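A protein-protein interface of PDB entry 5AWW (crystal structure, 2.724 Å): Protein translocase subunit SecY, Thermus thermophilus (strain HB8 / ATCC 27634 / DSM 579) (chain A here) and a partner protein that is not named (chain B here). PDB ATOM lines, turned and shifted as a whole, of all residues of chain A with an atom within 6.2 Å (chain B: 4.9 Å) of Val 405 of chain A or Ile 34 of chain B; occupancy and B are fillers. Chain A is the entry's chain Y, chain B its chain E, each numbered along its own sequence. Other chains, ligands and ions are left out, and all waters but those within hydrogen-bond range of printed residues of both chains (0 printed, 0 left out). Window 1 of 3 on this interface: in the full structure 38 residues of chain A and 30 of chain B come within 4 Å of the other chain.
CG of Met 1 of chain A touches CB of Ala 33 of chain B, at 3.6 Å. CE1 of Phe 37 of chain B touches CZ of Phe 189 of chain A, 3.6 Å away. Phe 228 of chain A touches Ile 34 of chain B (CD2 to CG2, 3.8 Å). Phe 228 of chain A touches Leu 35 of chain B (CD2 to CD2, 3.6 Å). OG1 of Thr 31 of chain B touches CA of Ala 229 of chain A, 3.3 Å away. Val 404 of chain A touches Thr 38 of chain B (CG1 to OG1, 3.4 Å). CB of Ala 408 of chain A touches CD1 of Phe 37 of chain B, at 3.5 Å. CD1 of Ile 34 of chain B touches CD2 of Leu 409 of chain A, at 3.7 Å. CD1 of Leu 412 of chain A touches CB of Ala 33 of chain B, at 3.6 Å. Leu 412 of chain A touches Phe 37 of chain B (CD2 to CD2, 3.9 Å).
Of the 20 printed residues of chain A, 9 touch a printed residue of chain B. Printed residues of chain A that touch a printed residue of chain B: Met 1, Phe 189, Phe 228, Ala 229, Val 404, Val 405, Ala 408, Leu 409 and Leu 412. Hydrophobic or aromatic side chains of chain A within 4 Å of the printed part of chain B: Met 1, Phe 189, Phe 228, Ala 229, Val 404, Val 405, Ala 408, Leu 409 and Leu 412. Printed residues of chain B that touch a printed residue of chain A: Thr 31, Ala 33, Ile 34, Leu 35, Phe 37 and Thr 38. Hydrophobic or aromatic side chains of chain B that line the printed part of chain A: Ala 33, Ile 34, Leu 35 and Phe 37.
Printed residues of chain B within 4 Å of Met 1 of chain A: Ala 33 (3.6 Å). Ala 227 of chain A touches none of the printed residues of chain B. Val 405 of chain A touches one residue of chain B. Printed residues of chain A within 4 Å of Thr 31 of chain B: Ala 229 (3.3 Å). Printed residues of chain A within 4 Å of Phe 37 of chain B: Phe 189 (3.6 Å), Ala 408 (3.5 Å) and Leu 412 (3.9 Å). Of the printed residues of chain A, Thr 38 of chain B touches Val 404 (3.4 Å). The nearest printed residue of chain B that does not touch Val 405 of chain A is Thr 38 of chain B (5.7 Å). The nearest printed residue of chain B that does not touch Met 1 of chain A is Gly 30 of chain B (4.5 Å).
O of Ile 34 of chain B sits at hydrogen-bond distance from OG1 of Thr 38 of chain B, at 3.0 Å.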
ATOM      1  N   MET A   1       5.940   6.204  -6.784  1.00  0.00           N
ATOM      2  CA  MET A   1       7.026   5.242  -6.931  1.00  0.00           C
ATOM      3  C   MET A   1       6.492   3.813  -7.018  1.00  0.00           C
ATOM      4  O   MET A   1       7.263   2.856  -7.091  1.00  0.00           O
ATOM      5  CB  MET A   1       8.019   5.376  -5.774  1.00  0.00           C
ATOM      6  CG  MET A   1       7.384   5.354  -4.394  1.00  0.00           C
ATOM      7  SD  MET A   1       8.558   5.769  -3.087  1.00  0.00           S
ATOM      8  CE  MET A   1       8.949   7.465  -3.506  1.00  0.00           C
ATOM      9  N   PHE A 189      18.798  -6.410   4.210  1.00  0.00           N
ATOM     10  CA  PHE A 189      17.351  -6.366   4.032  1.00  0.00           C
ATOM     11  C   PHE A 189      16.759  -7.766   3.973  1.00  0.00           C
ATOM     12  O   PHE A 189      15.837  -8.088   4.723  1.00  0.00           O
ATOM     13  CB  PHE A 189      16.997  -5.592   2.757  1.00  0.00           C
ATOM     14  CG  PHE A 189      15.531  -5.593   2.427  1.00  0.00           C
ATOM     15  CD1 PHE A 189      14.678  -4.671   3.008  1.00  0.00           C
ATOM     16  CD2 PHE A 189      15.008  -6.504   1.522  1.00  0.00           C
ATOM     17  CE1 PHE A 189      13.329  -4.666   2.702  1.00  0.00           C
ATOM     18  CE2 PHE A 189      13.661  -6.503   1.215  1.00  0.00           C
ATOM     19  CZ  PHE A 189      12.821  -5.582   1.805  1.00  0.00           C
ATOM     20  N   ALA A 227       4.234   2.967  11.184  1.00  0.00           N
ATOM     21  CA  ALA A 227       5.666   3.180  11.029  1.00  0.00           C
ATOM     22  C   ALA A 227       6.007   3.414   9.567  1.00  0.00           C
ATOM     23  O   ALA A 227       6.714   4.370   9.226  1.00  0.00           O
ATOM     24  CB  ALA A 227       6.445   1.992  11.578  1.00  0.00           C
ATOM     25  N   PHE A 228       5.489   2.539   8.708  1.00  0.00           N
ATOM     26  CA  PHE A 228       5.706   2.663   7.269  1.00  0.00           C
ATOM     27  C   PHE A 228       5.203   4.007   6.749  1.00  0.00           C
ATOM     28  O   PHE A 228       5.939   4.747   6.092  1.00  0.00           O
ATOM     29  CB  PHE A 228       5.014   1.526   6.515  1.00  0.00           C
ATOM     30  CG  PHE A 228       5.686   0.191   6.667  1.00  0.00           C
ATOM     31  CD1 PHE A 228       6.777   0.036   7.505  1.00  0.00           C
ATOM     32  CD2 PHE A 228       5.235  -0.909   5.957  1.00  0.00           C
ATOM     33  CE1 PHE A 228       7.397  -1.191   7.641  1.00  0.00           C
ATOM     34  CE2 PHE A 228       5.852  -2.136   6.087  1.00  0.00           C
ATOM     35  CZ  PHE A 228       6.933  -2.277   6.930  1.00  0.00           C
ATOM     36  N   ALA A 229       3.947   4.315   7.058  1.00  0.00           N
ATOM     37  CA  ALA A 229       3.319   5.554   6.618  1.00  0.00           C
ATOM     38  C   ALA A 229       4.067   6.786   7.122  1.00  0.00           C
ATOM     39  O   ALA A 229       4.238   7.760   6.392  1.00  0.00           O
ATOM     40  CB  ALA A 229       1.868   5.595   7.076  1.00  0.00           C
ATOM     41  N   MET A 231       7.337   7.040   8.142  1.00  0.00           N
ATOM     42  CA  MET A 231       8.629   7.154   7.474  1.00  0.00           C
ATOM     43  C   MET A 231       8.462   7.633   6.033  1.00  0.00           C
ATOM     44  O   MET A 231       9.265   8.425   5.538  1.00  0.00           O
ATOM     45  CB  MET A 231       9.371   5.816   7.507  1.00  0.00           C
ATOM     46  CG  MET A 231       9.794   5.387   8.900  1.00  0.00           C
ATOM     47  SD  MET A 231      10.865   3.942   8.879  1.00  0.00           S
ATOM     48  CE  MET A 231      12.295   4.606   8.021  1.00  0.00           C
ATOM     49  N   ALA A 232       7.410   7.155   5.375  1.00  0.00           N
ATOM     50  CA  ALA A 232       7.100   7.568   4.010  1.00  0.00           C
ATOM     51  C   ALA A 232       6.801   9.061   3.948  1.00  0.00           C
ATOM     52  O   ALA A 232       7.324   9.781   3.090  1.00  0.00           O
ATOM     53  CB  ALA A 232       5.925   6.770   3.471  1.00  0.00           C
ATOM     54  N   VAL A 271      20.244   4.498   3.754  1.00  0.00           N
ATOM     55  CA  VAL A 271      20.030   3.673   4.933  1.00  0.00           C
ATOM     56  C   VAL A 271      21.370   3.394   5.615  1.00  0.00           C
ATOM     57  O   VAL A 271      21.427   2.768   6.674  1.00  0.00           O
ATOM     58  CB  VAL A 271      19.327   2.347   4.568  1.00  0.00           C
ATOM     59  CG1 VAL A 271      20.319   1.369   3.955  1.00  0.00           C
ATOM     60  CG2 VAL A 271      18.642   1.736   5.788  1.00  0.00           C
ATOM     61  N   GLY A 400      15.201  -2.607  12.814  1.00  0.00           N
ATOM     62  CA  GLY A 400      14.819  -3.475  11.715  1.00  0.00           C
ATOM     63  C   GLY A 400      13.890  -2.773  10.747  1.00  0.00           C
ATOM     64  O   GLY A 400      14.078  -2.845   9.530  1.00  0.00           O
ATOM     65  N   LEU A 401      12.881  -2.099  11.292  1.00  0.00           N
ATOM     66  CA  LEU A 401      11.959  -1.305  10.488  1.00  0.00           C
ATOM     67  C   LEU A 401      12.725  -0.254   9.699  1.00  0.00           C
ATOM     68  O   LEU A 401      12.501  -0.079   8.498  1.00  0.00           O
ATOM     69  CB  LEU A 401      10.905  -0.636  11.371  1.00  0.00           C
ATOM     70  CG  LEU A 401       9.970  -1.581  12.125  1.00  0.00           C
ATOM     71  CD1 LEU A 401       9.048  -0.802  13.053  1.00  0.00           C
ATOM     72  CD2 LEU A 401       9.167  -2.422  11.145  1.00  0.00           C
ATOM     73  N   LEU A 402      13.634   0.438  10.384  1.00  0.00           N
ATOM     74  CA  LEU A 402      14.485   1.430   9.740  1.00  0.00           C
ATOM     75  C   LEU A 402      15.217   0.826   8.546  1.00  0.00           C
ATOM     76  O   LEU A 402      15.265   1.429   7.473  1.00  0.00           O
ATOM     77  CB  LEU A 402      15.487   2.012  10.737  1.00  0.00           C
ATOM     78  CG  LEU A 402      14.946   3.056  11.715  1.00  0.00           C
ATOM     79  CD1 LEU A 402      16.040   3.527  12.661  1.00  0.00           C
ATOM     80  CD2 LEU A 402      14.345   4.231  10.968  1.00  0.00           C
ATOM     81  N   ILE A 403      15.770  -0.371   8.728  1.00  0.00           N
ATOM     82  CA  ILE A 403      16.459  -1.057   7.635  1.00  0.00           C
ATOM     83  C   ILE A 403      15.524  -1.365   6.465  1.00  0.00           C
ATOM     84  O   ILE A 403      15.822  -1.024   5.319  1.00  0.00           O
ATOM     85  CB  ILE A 403      17.103  -2.373   8.101  1.00  0.00           C
ATOM     86  CG1 ILE A 403      18.160  -2.097   9.168  1.00  0.00           C
ATOM     87  CG2 ILE A 403      17.731  -3.104   6.923  1.00  0.00           C
ATOM     88  CD1 ILE A 403      19.180  -1.076   8.747  1.00  0.00           C
ATOM     89  N   VAL A 404      14.398  -2.007   6.760  1.00  0.00           N
ATOM     90  CA  VAL A 404      13.454  -2.422   5.724  1.00  0.00           C
ATOM     91  C   VAL A 404      12.927  -1.237   4.914  1.00  0.00           C
ATOM     92  O   VAL A 404      13.062  -1.198   3.686  1.00  0.00           O
ATOM     93  CB  VAL A 404      12.265  -3.185   6.335  1.00  0.00           C
ATOM     94  CG1 VAL A 404      11.216  -3.482   5.275  1.00  0.00           C
ATOM     95  CG2 VAL A 404      12.744  -4.465   6.997  1.00  0.00           C
ATOM     96  N   VAL A 405      12.331  -0.273   5.607  1.00  0.00           N
ATOM     97  CA  VAL A 405      11.775   0.907   4.956  1.00  0.00           C
ATOM     98  C   VAL A 405      12.864   1.700   4.243  1.00  0.00           C
ATOM     99  O   VAL A 405      12.650   2.219   3.147  1.00  0.00           O
ATOM    100  CB  VAL A 405      11.058   1.819   5.966  1.00  0.00           C
ATOM    101  CG1 VAL A 405      10.470   3.037   5.266  1.00  0.00           C
ATOM    102  CG2 VAL A 405       9.974   1.050   6.688  1.00  0.00           C
ATOM    103  N   GLY A 406      14.034   1.778   4.866  1.00  0.00           N
ATOM    104  CA  GLY A 406      15.161   2.480   4.283  1.00  0.00           C
ATOM    105  C   GLY A 406      15.552   1.903   2.939  1.00  0.00           C
ATOM    106  O   GLY A 406      15.582   2.613   1.935  1.00  0.00           O
ATOM    107  N   VAL A 407      15.835   0.605   2.923  1.00  0.00           N
ATOM    108  CA  VAL A 407      16.254  -0.080   1.707  1.00  0.00           C
ATOM    109  C   VAL A 407      15.173  -0.031   0.633  1.00  0.00           C
ATOM    110  O   VAL A 407      15.463   0.251  -0.534  1.00  0.00           O
ATOM    111  CB  VAL A 407      16.625  -1.544   1.994  1.00  0.00           C
ATOM    112  CG1 VAL A 407      16.866  -2.301   0.698  1.00  0.00           C
ATOM    113  CG2 VAL A 407      17.855  -1.607   2.887  1.00  0.00           C
ATOM    114  N   ALA A 408      13.931  -0.298   1.030  1.00  0.00           N
ATOM    115  CA  ALA A 408      12.805  -0.250   0.098  1.00  0.00           C
ATOM    116  C   ALA A 408      12.712   1.117  -0.579  1.00  0.00           C
ATOM    117  O   ALA A 408      12.725   1.220  -1.813  1.00  0.00           O
ATOM    118  CB  ALA A 408      11.509  -0.573   0.819  1.00  0.00           C
ATOM    119  N   LEU A 409      12.636   2.162   0.242  1.00  0.00           N
ATOM    120  CA  LEU A 409      12.545   3.528  -0.257  1.00  0.00           C
ATOM    121  C   LEU A 409      13.726   3.886  -1.153  1.00  0.00           C
ATOM    122  O   LEU A 409      13.538   4.498  -2.193  1.00  0.00           O
ATOM    123  CB  LEU A 409      12.447   4.522   0.905  1.00  0.00           C
ATOM    124  CG  LEU A 409      11.087   4.617   1.601  1.00  0.00           C
ATOM    125  CD1 LEU A 409      11.113   5.662   2.707  1.00  0.00           C
ATOM    126  CD2 LEU A 409       9.988   4.925   0.595  1.00  0.00           C
ATOM    127  N   ASP A 410      14.935   3.498  -0.755  1.00  0.00           N
ATOM    128  CA  ASP A 410      16.131   3.784  -1.550  1.00  0.00           C
ATOM    129  C   ASP A 410      16.082   3.128  -2.929  1.00  0.00           C
ATOM    130  O   ASP A 410      16.310   3.785  -3.951  1.00  0.00           O
ATOM    131  CB  ASP A 410      17.391   3.322  -0.812  1.00  0.00           C
ATOM    132  CG  ASP A 410      17.806   4.278   0.288  1.00  0.00           C
ATOM    133  OD1 ASP A 410      16.923   4.957   0.854  1.00  0.00           O
ATOM    134  OD2 ASP A 410      19.017   4.349   0.587  1.00  0.00           O
ATOM    135  N   LEU A 412      13.456   1.850  -4.600  1.00  0.00           N
ATOM    136  CA  LEU A 412      12.363   2.389  -5.403  1.00  0.00           C
ATOM    137  C   LEU A 412      12.659   3.805  -5.897  1.00  0.00           C
ATOM    138  O   LEU A 412      12.307   4.168  -7.022  1.00  0.00           O
ATOM    139  CB  LEU A 412      11.061   2.379  -4.605  1.00  0.00           C
ATOM    140  CG  LEU A 412      10.514   0.992  -4.264  1.00  0.00           C
ATOM    141  CD1 LEU A 412       9.275   1.104  -3.393  1.00  0.00           C
ATOM    142  CD2 LEU A 412      10.211   0.210  -5.534  1.00  0.00           C
ATOM    143  N   GLY B  30       3.695   6.306  -1.266  1.00  0.00           N
ATOM    144  CA  GLY B  30       4.874   5.807  -0.584  1.00  0.00           C
ATOM    145  C   GLY B  30       4.586   4.569   0.240  1.00  0.00           C
ATOM    146  O   GLY B  30       5.310   3.576   0.152  1.00  0.00           O
ATOM    147  N   THR B  31       3.519   4.622   1.030  1.00  0.00           N
ATOM    148  CA  THR B  31       3.160   3.500   1.890  1.00  0.00           C
ATOM    149  C   THR B  31       2.821   2.254   1.073  1.00  0.00           C
ATOM    150  O   THR B  31       3.269   1.155   1.398  1.00  0.00           O
ATOM    151  CB  THR B  31       1.973   3.851   2.807  1.00  0.00           C
ATOM    152  OG1 THR B  31       2.273   5.044   3.541  1.00  0.00           O
ATOM    153  CG2 THR B  31       1.701   2.716   3.782  1.00  0.00           C
ATOM    154  N   GLN B  32       2.041   2.429   0.010  1.00  0.00           N
ATOM    155  CA  GLN B  32       1.686   1.315  -0.869  1.00  0.00           C
ATOM    156  C   GLN B  32       2.926   0.707  -1.514  1.00  0.00           C
ATOM    157  O   GLN B  32       3.049  -0.515  -1.619  1.00  0.00           O
ATOM    158  CB  GLN B  32       0.702   1.771  -1.950  1.00  0.00           C
ATOM    159  CG  GLN B  32      -0.712   2.002  -1.442  1.00  0.00           C
ATOM    160  CD  GLN B  32      -1.631   2.575  -2.505  1.00  0.00           C
ATOM    161  OE1 GLN B  32      -1.176   3.132  -3.503  1.00  0.00           O
ATOM    162  NE2 GLN B  32      -2.935   2.440  -2.293  1.00  0.00           N
ATOM    163  N   ALA B  33       3.842   1.570  -1.942  1.00  0.00           N
ATOM    164  CA  ALA B  33       5.096   1.131  -2.539  1.00  0.00           C
ATOM    165  C   ALA B  33       5.905   0.287  -1.557  1.00  0.00           C
ATOM    166  O   ALA B  33       6.346  -0.817  -1.887  1.00  0.00           O
ATOM    167  CB  ALA B  33       5.904   2.329  -3.003  1.00  0.00           C
ATOM    168  N   ILE B  34       6.091   0.820  -0.353  1.00  0.00           N
ATOM    169  CA  ILE B  34       6.829   0.126   0.697  1.00  0.00           C
ATOM    170  C   ILE B  34       6.206  -1.234   0.994  1.00  0.00           C
ATOM    171  O   ILE B  34       6.909  -2.245   1.107  1.00  0.00           O
ATOM    172  CB  ILE B  34       6.880   0.968   1.994  1.00  0.00           C
ATOM    173  CG1 ILE B  34       7.680   2.252   1.759  1.00  0.00           C
ATOM    174  CG2 ILE B  34       7.492   0.170   3.135  1.00  0.00           C
ATOM    175  CD1 ILE B  34       7.680   3.196   2.935  1.00  0.00           C
ATOM    176  N   LEU B  35       4.880  -1.252   1.099  1.00  0.00           N
ATOM    177  CA  LEU B  35       4.149  -2.485   1.364  1.00  0.00           C
ATOM    178  C   LEU B  35       4.364  -3.513   0.255  1.00  0.00           C
ATOM    179  O   LEU B  35       4.636  -4.676   0.532  1.00  0.00           O
ATOM    180  CB  LEU B  35       2.656  -2.197   1.538  1.00  0.00           C
ATOM    181  CG  LEU B  35       2.257  -1.465   2.822  1.00  0.00           C
ATOM    182  CD1 LEU B  35       0.783  -1.086   2.799  1.00  0.00           C
ATOM    183  CD2 LEU B  35       2.575  -2.307   4.048  1.00  0.00           C
ATOM    184  N   LEU B  36       4.250  -3.079  -0.997  1.00  0.00           N
ATOM    185  CA  LEU B  36       4.455  -3.974  -2.134  1.00  0.00           C
ATOM    186  C   LEU B  36       5.863  -4.561  -2.139  1.00  0.00           C
ATOM    187  O   LEU B  36       6.031  -5.768  -2.265  1.00  0.00           O
ATOM    188  CB  LEU B  36       4.191  -3.243  -3.451  1.00  0.00           C
ATOM    189  CG  LEU B  36       2.718  -2.990  -3.767  1.00  0.00           C
ATOM    190  CD1 LEU B  36       2.572  -2.149  -5.024  1.00  0.00           C
ATOM    191  CD2 LEU B  36       1.974  -4.310  -3.910  1.00  0.00           C
ATOM    192  N   PHE B  37       6.863  -3.696  -1.998  1.00  0.00           N
ATOM    193  CA  PHE B  37       8.261  -4.114  -1.932  1.00  0.00           C
ATOM    194  C   PHE B  37       8.483  -5.179  -0.851  1.00  0.00           C
ATOM    195  O   PHE B  37       8.901  -6.319  -1.136  1.00  0.00           O
ATOM    196  CB  PHE B  37       9.144  -2.890  -1.661  1.00  0.00           C
ATOM    197  CG  PHE B  37      10.599  -3.101  -1.960  1.00  0.00           C
ATOM    198  CD1 PHE B  37      11.460  -3.585  -0.987  1.00  0.00           C
ATOM    199  CD2 PHE B  37      11.111  -2.794  -3.211  1.00  0.00           C
ATOM    200  CE1 PHE B  37      12.803  -3.769  -1.260  1.00  0.00           C
ATOM    201  CE2 PHE B  37      12.453  -2.977  -3.490  1.00  0.00           C
ATOM    202  CZ  PHE B  37      13.300  -3.465  -2.513  1.00  0.00           C
ATOM    203  N   THR B  38       8.180  -4.795   0.387  1.00  0.00           N
ATOM    204  CA  THR B  38       8.387  -5.660   1.541  1.00  0.00           C
ATOM    205  C   THR B  38       7.652  -6.988   1.395  1.00  0.00           C
ATOM    206  O   THR B  38       8.243  -8.048   1.586  1.00  0.00           O
ATOM    207  CB  THR B  38       7.933  -4.975   2.843  1.00  0.00           C
ATOM    208  OG1 THR B  38       8.654  -3.749   3.017  1.00  0.00           O
ATOM    209  CG2 THR B  38       8.185  -5.880   4.039  1.00  0.00           C
ATOM    210  N   LEU B  39       6.369  -6.924   1.050  1.00  0.00           N
ATOM    211  CA  LEU B  39       5.555  -8.125   0.883  1.00  0.00           C
ATOM    212  C   LEU B  39       6.122  -9.036  -0.202  1.00  0.00           C
ATOM    213  O   LEU B  39       6.164 -10.257  -0.040  1.00  0.00           O
ATOM    214  CB  LEU B  39       4.110  -7.752   0.549  1.00  0.00           C
ATOM    215  CG  LEU B  39       3.138  -8.909   0.313  1.00  0.00           C
ATOM    216  CD1 LEU B  39       2.986  -9.751   1.571  1.00  0.00           C
ATOM    217  CD2 LEU B  39       1.790  -8.390  -0.161  1.00  0.00           C
